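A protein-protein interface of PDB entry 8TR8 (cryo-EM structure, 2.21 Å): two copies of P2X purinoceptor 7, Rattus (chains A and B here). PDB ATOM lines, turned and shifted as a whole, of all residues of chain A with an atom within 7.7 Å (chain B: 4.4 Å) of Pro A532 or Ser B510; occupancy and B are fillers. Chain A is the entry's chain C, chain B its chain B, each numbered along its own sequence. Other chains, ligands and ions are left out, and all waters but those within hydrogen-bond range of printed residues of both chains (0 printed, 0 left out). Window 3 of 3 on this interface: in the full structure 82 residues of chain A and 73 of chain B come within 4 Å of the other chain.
The backbone carbonyl oxygen (O) of Tyr A529 lies within hydrogen-bond range of the indole nitrogen (NE1) of Trp B556, at 3.1 Å.
Leu A526 touches none of the printed residues of chain B.
Of the printed residues of chain B, Leu A528 touches Leu B512.
Of chain B, only Ser B510, Trp B556 and Arg B557 come within 4 Å of Pro A532.
Of the printed residues of chain A, Val B404 touches Leu A533 (3.6 Å).
Ser B510 touches one residue of chain A.
Of the printed residues of chain A, Leu B512 touches Leu A528.
Ser B514 touches none of the printed residues of chain A.
Printed residues of chain A within 4 Å of Trp B556: Tyr A529 and Pro A532.
Of the printed residues of chain A, Arg B557 touches Tyr A529 (3.8 Å) and Pro A532 (3.6 Å).
The nearest printed residue of chain A that does not touch Arg B557 is Gln A530 (4.6 Å).
No position is printed for both chains.
Of the 7 pairs that touch across the chains among the printed residues, none has its exchanged pair printed and touching as well.
Among the printed residues, pairs that only touch across the chains: Leu A533 with Val B404 (3.6 Å), Pro A532 with Arg B557 (3.6 Å), Pro A532 with Ser B510 (3.6 Å), Leu A528 with Leu B512 (3.6 Å), Tyr A529 with Arg B557 (3.8 Å) and Pro A532 with Trp B556 (3.8 Å).
Of the 11 printed residues of chain B, 5 touch a printed residue of chain A.
Hydrophobic or aromatic side chains of chain B that line the printed part of chain A: Val B404, Leu B512 and Trp B556.
Hydrophobic or aromatic side chains of chain A within 4 Å of the printed part of chain B: Leu A528, Tyr A529, Pro A532 and Leu A533.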
ATOM      1  N   LEU A 526     -29.825 -15.084  -8.722  1.00  0.00           N
ATOM      2  CA  LEU A 526     -30.336 -15.483  -7.412  1.00  0.00           C
ATOM      3  C   LEU A 526     -31.299 -16.657  -7.537  1.00  0.00           C
ATOM      4  O   LEU A 526     -31.210 -17.638  -6.783  1.00  0.00           O
ATOM      5  CB  LEU A 526     -31.018 -14.304  -6.717  1.00  0.00           C
ATOM      6  CG  LEU A 526     -30.264 -12.983  -6.594  1.00  0.00           C
ATOM      7  CD1 LEU A 526     -31.219 -11.887  -6.174  1.00  0.00           C
ATOM      8  CD2 LEU A 526     -29.122 -13.092  -5.607  1.00  0.00           C
ATOM      9  N   LEU A 527     -32.223 -16.583  -8.496  1.00  0.00           N
ATOM     10  CA  LEU A 527     -33.183 -17.667  -8.674  1.00  0.00           C
ATOM     11  C   LEU A 527     -32.480 -18.973  -9.013  1.00  0.00           C
ATOM     12  O   LEU A 527     -32.834 -20.032  -8.484  1.00  0.00           O
ATOM     13  CB  LEU A 527     -34.188 -17.301  -9.760  1.00  0.00           C
ATOM     14  CG  LEU A 527     -35.138 -16.147  -9.434  1.00  0.00           C
ATOM     15  CD1 LEU A 527     -35.982 -15.801 -10.640  1.00  0.00           C
ATOM     16  CD2 LEU A 527     -36.020 -16.486  -8.245  1.00  0.00           C
ATOM     17  N   LEU A 528     -31.481 -18.916  -9.894  1.00  0.00           N
ATOM     18  CA  LEU A 528     -30.744 -20.121 -10.254  1.00  0.00           C
ATOM     19  C   LEU A 528     -29.971 -20.670  -9.063  1.00  0.00           C
ATOM     20  O   LEU A 528     -29.850 -21.888  -8.902  1.00  0.00           O
ATOM     21  CB  LEU A 528     -29.806 -19.827 -11.422  1.00  0.00           C
ATOM     22  CG  LEU A 528     -30.456 -19.655 -12.798  1.00  0.00           C
ATOM     23  CD1 LEU A 528     -29.393 -19.630 -13.864  1.00  0.00           C
ATOM     24  CD2 LEU A 528     -31.465 -20.754 -13.089  1.00  0.00           C
ATOM     25  N   TYR A 529     -29.435 -19.787  -8.220  1.00  0.00           N
ATOM     26  CA  TYR A 529     -28.829 -20.244  -6.977  1.00  0.00           C
ATOM     27  C   TYR A 529     -29.840 -21.012  -6.138  1.00  0.00           C
ATOM     28  O   TYR A 529     -29.513 -22.051  -5.552  1.00  0.00           O
ATOM     29  CB  TYR A 529     -28.270 -19.059  -6.194  1.00  0.00           C
ATOM     30  CG  TYR A 529     -27.282 -19.431  -5.114  1.00  0.00           C
ATOM     31  CD1 TYR A 529     -27.713 -19.826  -3.857  1.00  0.00           C
ATOM     32  CD2 TYR A 529     -25.918 -19.382  -5.348  1.00  0.00           C
ATOM     33  CE1 TYR A 529     -26.817 -20.162  -2.870  1.00  0.00           C
ATOM     34  CE2 TYR A 529     -25.014 -19.716  -4.364  1.00  0.00           C
ATOM     35  CZ  TYR A 529     -25.469 -20.108  -3.127  1.00  0.00           C
ATOM     36  OH  TYR A 529     -24.577 -20.444  -2.137  1.00  0.00           O
ATOM     37  N   GLN A 530     -31.077 -20.516  -6.065  1.00  0.00           N
ATOM     38  CA  GLN A 530     -32.114 -21.255  -5.351  1.00  0.00           C
ATOM     39  C   GLN A 530     -32.589 -22.463  -6.153  1.00  0.00           C
ATOM     40  O   GLN A 530     -32.815 -23.538  -5.587  1.00  0.00           O
ATOM     41  CB  GLN A 530     -33.291 -20.337  -5.028  1.00  0.00           C
ATOM     42  CG  GLN A 530     -32.906 -19.031  -4.353  1.00  0.00           C
ATOM     43  CD  GLN A 530     -31.872 -19.216  -3.264  1.00  0.00           C
ATOM     44  OE1 GLN A 530     -30.689 -18.936  -3.459  1.00  0.00           O
ATOM     45  NE2 GLN A 530     -32.313 -19.689  -2.108  1.00  0.00           N
ATOM     46  N   GLU A 531     -32.749 -22.306  -7.468  1.00  0.00           N
ATOM     47  CA  GLU A 531     -33.244 -23.364  -8.349  1.00  0.00           C
ATOM     48  C   GLU A 531     -32.275 -23.538  -9.510  1.00  0.00           C
ATOM     49  O   GLU A 531     -32.395 -22.857 -10.535  1.00  0.00           O
ATOM     50  CB  GLU A 531     -34.647 -23.048  -8.858  1.00  0.00           C
ATOM     51  CG  GLU A 531     -35.748 -23.314  -7.855  1.00  0.00           C
ATOM     52  CD  GLU A 531     -36.491 -22.056  -7.456  1.00  0.00           C
ATOM     53  OE1 GLU A 531     -35.832 -21.017  -7.234  1.00  0.00           O
ATOM     54  OE2 GLU A 531     -37.735 -22.104  -7.364  1.00  0.00           O
ATOM     55  N   PRO A 532     -31.309 -24.452  -9.393  1.00  0.00           N
ATOM     56  CA  PRO A 532     -30.263 -24.539 -10.426  1.00  0.00           C
ATOM     57  C   PRO A 532     -30.795 -24.798 -11.824  1.00  0.00           C
ATOM     58  O   PRO A 532     -30.216 -24.297 -12.796  1.00  0.00           O
ATOM     59  CB  PRO A 532     -29.383 -25.698  -9.935  1.00  0.00           C
ATOM     60  CG  PRO A 532     -29.684 -25.831  -8.495  1.00  0.00           C
ATOM     61  CD  PRO A 532     -31.103 -25.438  -8.321  1.00  0.00           C
ATOM     62  N   LEU A 533     -31.872 -25.564 -11.961  1.00  0.00           N
ATOM     63  CA  LEU A 533     -32.412 -25.950 -13.259  1.00  0.00           C
ATOM     64  C   LEU A 533     -33.744 -25.262 -13.539  1.00  0.00           C
ATOM     65  O   LEU A 533     -34.648 -25.842 -14.141  1.00  0.00           O
ATOM     66  CB  LEU A 533     -32.569 -27.466 -13.344  1.00  0.00           C
ATOM     67  CG  LEU A 533     -31.290 -28.285 -13.183  1.00  0.00           C
ATOM     68  CD1 LEU A 533     -31.617 -29.762 -13.139  1.00  0.00           C
ATOM     69  CD2 LEU A 533     -30.306 -27.991 -14.300  1.00  0.00           C
ATOM     70  N   LEU A 534     -33.874 -24.012 -13.106  1.00  0.00           N
ATOM     71  CA  LEU A 534     -35.089 -23.255 -13.356  1.00  0.00           C
ATOM     72  C   LEU A 534     -35.200 -22.893 -14.832  1.00  0.00           C
ATOM     73  O   LEU A 534     -34.198 -22.669 -15.518  1.00  0.00           O
ATOM     74  CB  LEU A 534     -35.111 -21.989 -12.502  1.00  0.00           C
ATOM     75  CG  LEU A 534     -36.440 -21.235 -12.458  1.00  0.00           C
ATOM     76  CD1 LEU A 534     -37.522 -22.083 -11.816  1.00  0.00           C
ATOM     77  CD2 LEU A 534     -36.272 -19.926 -11.714  1.00  0.00           C
ATOM     78  N   ALA A 535     -36.435 -22.839 -15.318  1.00  0.00           N
ATOM     79  CA  ALA A 535     -36.723 -22.535 -16.713  1.00  0.00           C
ATOM     80  C   ALA A 535     -37.074 -21.057 -16.841  1.00  0.00           C
ATOM     81  O   ALA A 535     -38.033 -20.587 -16.220  1.00  0.00           O
ATOM     82  CB  ALA A 535     -37.861 -23.406 -17.235  1.00  0.00           C
ATOM     83  N   VAL B 404     -30.912 -32.504  -7.264  1.00  0.00           N
ATOM     84  CA  VAL B 404     -31.430 -31.318  -7.932  1.00  0.00           C
ATOM     85  C   VAL B 404     -32.927 -31.444  -8.165  1.00  0.00           C
ATOM     86  O   VAL B 404     -33.638 -30.435  -8.257  1.00  0.00           O
ATOM     87  CB  VAL B 404     -30.659 -31.084  -9.245  1.00  0.00           C
ATOM     88  CG1 VAL B 404     -31.155 -32.021 -10.334  1.00  0.00           C
ATOM     89  CG2 VAL B 404     -30.768 -29.636  -9.667  1.00  0.00           C
ATOM     90  N   ILE B 507     -26.884 -31.442 -13.232  1.00  0.00           N
ATOM     91  CA  ILE B 507     -26.721 -30.120 -12.637  1.00  0.00           C
ATOM     92  C   ILE B 507     -25.540 -29.387 -13.256  1.00  0.00           C
ATOM     93  O   ILE B 507     -25.511 -28.151 -13.284  1.00  0.00           O
ATOM     94  CB  ILE B 507     -26.568 -30.244 -11.109  1.00  0.00           C
ATOM     95  CG1 ILE B 507     -26.541 -28.861 -10.462  1.00  0.00           C
ATOM     96  CG2 ILE B 507     -25.307 -31.018 -10.760  1.00  0.00           C
ATOM     97  CD1 ILE B 507     -26.780 -28.883  -8.980  1.00  0.00           C
ATOM     98  N   THR B 508     -24.548 -30.125 -13.757  1.00  0.00           N
ATOM     99  CA  THR B 508     -23.384 -29.498 -14.366  1.00  0.00           C
ATOM    100  C   THR B 508     -23.744 -28.639 -15.571  1.00  0.00           C
ATOM    101  O   THR B 508     -22.975 -27.739 -15.926  1.00  0.00           O
ATOM    102  CB  THR B 508     -22.373 -30.564 -14.790  1.00  0.00           C
ATOM    103  OG1 THR B 508     -22.988 -31.475 -15.704  1.00  0.00           O
ATOM    104  CG2 THR B 508     -21.865 -31.330 -13.587  1.00  0.00           C
ATOM    105  N   THR B 509     -24.887 -28.893 -16.210  1.00  0.00           N
ATOM    106  CA  THR B 509     -25.243 -28.132 -17.401  1.00  0.00           C
ATOM    107  C   THR B 509     -25.583 -26.687 -17.065  1.00  0.00           C
ATOM    108  O   THR B 509     -25.455 -25.806 -17.923  1.00  0.00           O
ATOM    109  CB  THR B 509     -26.418 -28.795 -18.118  1.00  0.00           C
ATOM    110  OG1 THR B 509     -27.607 -28.652 -17.334  1.00  0.00           O
ATOM    111  CG2 THR B 509     -26.140 -30.270 -18.344  1.00  0.00           C
ATOM    112  N   SER B 510     -26.011 -26.424 -15.835  1.00  0.00           N
ATOM    113  CA  SER B 510     -26.356 -25.067 -15.438  1.00  0.00           C
ATOM    114  C   SER B 510     -25.134 -24.162 -15.502  1.00  0.00           C
ATOM    115  O   SER B 510     -24.011 -24.582 -15.205  1.00  0.00           O
ATOM    116  CB  SER B 510     -26.939 -25.070 -14.029  1.00  0.00           C
ATOM    117  OG  SER B 510     -26.204 -25.934 -13.182  1.00  0.00           O
ATOM    118  N   GLU B 511     -25.354 -22.908 -15.904  1.00  0.00           N
ATOM    119  CA  GLU B 511     -24.259 -21.946 -15.948  1.00  0.00           C
ATOM    120  C   GLU B 511     -23.766 -21.604 -14.549  1.00  0.00           C
ATOM    121  O   GLU B 511     -22.596 -21.242 -14.373  1.00  0.00           O
ATOM    122  CB  GLU B 511     -24.700 -20.679 -16.678  1.00  0.00           C
ATOM    123  N   LEU B 512     -24.641 -21.711 -13.549  1.00  0.00           N
ATOM    124  CA  LEU B 512     -24.236 -21.437 -12.177  1.00  0.00           C
ATOM    125  C   LEU B 512     -23.152 -22.405 -11.725  1.00  0.00           C
ATOM    126  O   LEU B 512     -22.256 -22.035 -10.961  1.00  0.00           O
ATOM    127  CB  LEU B 512     -25.449 -21.520 -11.252  1.00  0.00           C
ATOM    128  CG  LEU B 512     -26.048 -20.202 -10.758  1.00  0.00           C
ATOM    129  CD1 LEU B 512     -25.179 -19.591  -9.688  1.00  0.00           C
ATOM    130  CD2 LEU B 512     -26.249 -19.224 -11.902  1.00  0.00           C
ATOM    131  N   PHE B 513     -23.221 -23.656 -12.186  1.00  0.00           N
ATOM    132  CA  PHE B 513     -22.213 -24.640 -11.814  1.00  0.00           C
ATOM    133  C   PHE B 513     -20.831 -24.211 -12.292  1.00  0.00           C
ATOM    134  O   PHE B 513     -19.851 -24.277 -11.543  1.00  0.00           O
ATOM    135  CB  PHE B 513     -22.587 -26.006 -12.391  1.00  0.00           C
ATOM    136  CG  PHE B 513     -21.693 -27.121 -11.942  1.00  0.00           C
ATOM    137  CD1 PHE B 513     -20.485 -27.351 -12.568  1.00  0.00           C
ATOM    138  CD2 PHE B 513     -22.061 -27.938 -10.893  1.00  0.00           C
ATOM    139  CE1 PHE B 513     -19.663 -28.371 -12.154  1.00  0.00           C
ATOM    140  CE2 PHE B 513     -21.246 -28.954 -10.478  1.00  0.00           C
ATOM    141  CZ  PHE B 513     -20.044 -29.174 -11.108  1.00  0.00           C
ATOM    142  N   SER B 514     -20.740 -23.764 -13.544  1.00  0.00           N
ATOM    143  CA  SER B 514     -19.458 -23.322 -14.080  1.00  0.00           C
ATOM    144  C   SER B 514     -19.002 -22.025 -13.427  1.00  0.00           C
ATOM    145  O   SER B 514     -17.808 -21.842 -13.169  1.00  0.00           O
ATOM    146  CB  SER B 514     -19.562 -23.159 -15.595  1.00  0.00           C
ATOM    147  OG  SER B 514     -20.400 -24.158 -16.152  1.00  0.00           O
ATOM    148  N   TRP B 556     -23.064 -24.171  -1.781  1.00  0.00           N
ATOM    149  CA  TRP B 556     -24.151 -23.772  -2.663  1.00  0.00           C
ATOM    150  C   TRP B 556     -25.366 -24.673  -2.489  1.00  0.00           C
ATOM    151  O   TRP B 556     -26.499 -24.192  -2.387  1.00  0.00           O
ATOM    152  CB  TRP B 556     -23.657 -23.791  -4.110  1.00  0.00           C
ATOM    153  CG  TRP B 556     -24.724 -23.639  -5.143  1.00  0.00           C
ATOM    154  CD1 TRP B 556     -25.887 -22.944  -5.025  1.00  0.00           C
ATOM    155  CD2 TRP B 556     -24.716 -24.191  -6.461  1.00  0.00           C
ATOM    156  NE1 TRP B 556     -26.611 -23.033  -6.188  1.00  0.00           N
ATOM    157  CE2 TRP B 556     -25.912 -23.794  -7.087  1.00  0.00           C
ATOM    158  CE3 TRP B 556     -23.815 -24.987  -7.174  1.00  0.00           C
ATOM    159  CZ2 TRP B 556     -26.229 -24.163  -8.389  1.00  0.00           C
ATOM    160  CZ3 TRP B 556     -24.132 -25.351  -8.468  1.00  0.00           C
ATOM    161  CH2 TRP B 556     -25.328 -24.940  -9.061  1.00  0.00           C
ATOM    162  N   ARG B 557     -25.153 -25.986  -2.444  1.00  0.00           N
ATOM    163  CA  ARG B 557     -26.265 -26.927  -2.406  1.00  0.00           C
ATOM    164  C   ARG B 557     -26.718 -27.282  -0.996  1.00  0.00           C
ATOM    165  O   ARG B 557     -27.757 -27.930  -0.845  1.00  0.00           O
ATOM    166  CB  ARG B 557     -25.893 -28.211  -3.155  1.00  0.00           C
ATOM    167  CG  ARG B 557     -25.424 -27.988  -4.579  1.00  0.00           C
ATOM    168  CD  ARG B 557     -26.407 -27.165  -5.386  1.00  0.00           C
ATOM    169  NE  ARG B 557     -27.751 -27.724  -5.347  1.00  0.00           N
ATOM    170  CZ  ARG B 557     -28.863 -27.022  -5.171  1.00  0.00           C
ATOM    171  NH1 ARG B 557     -28.840 -25.708  -5.020  1.00  0.00           N
ATOM    172  NH2 ARG B 557     -30.029 -27.656  -5.145  1.00  0.00           N
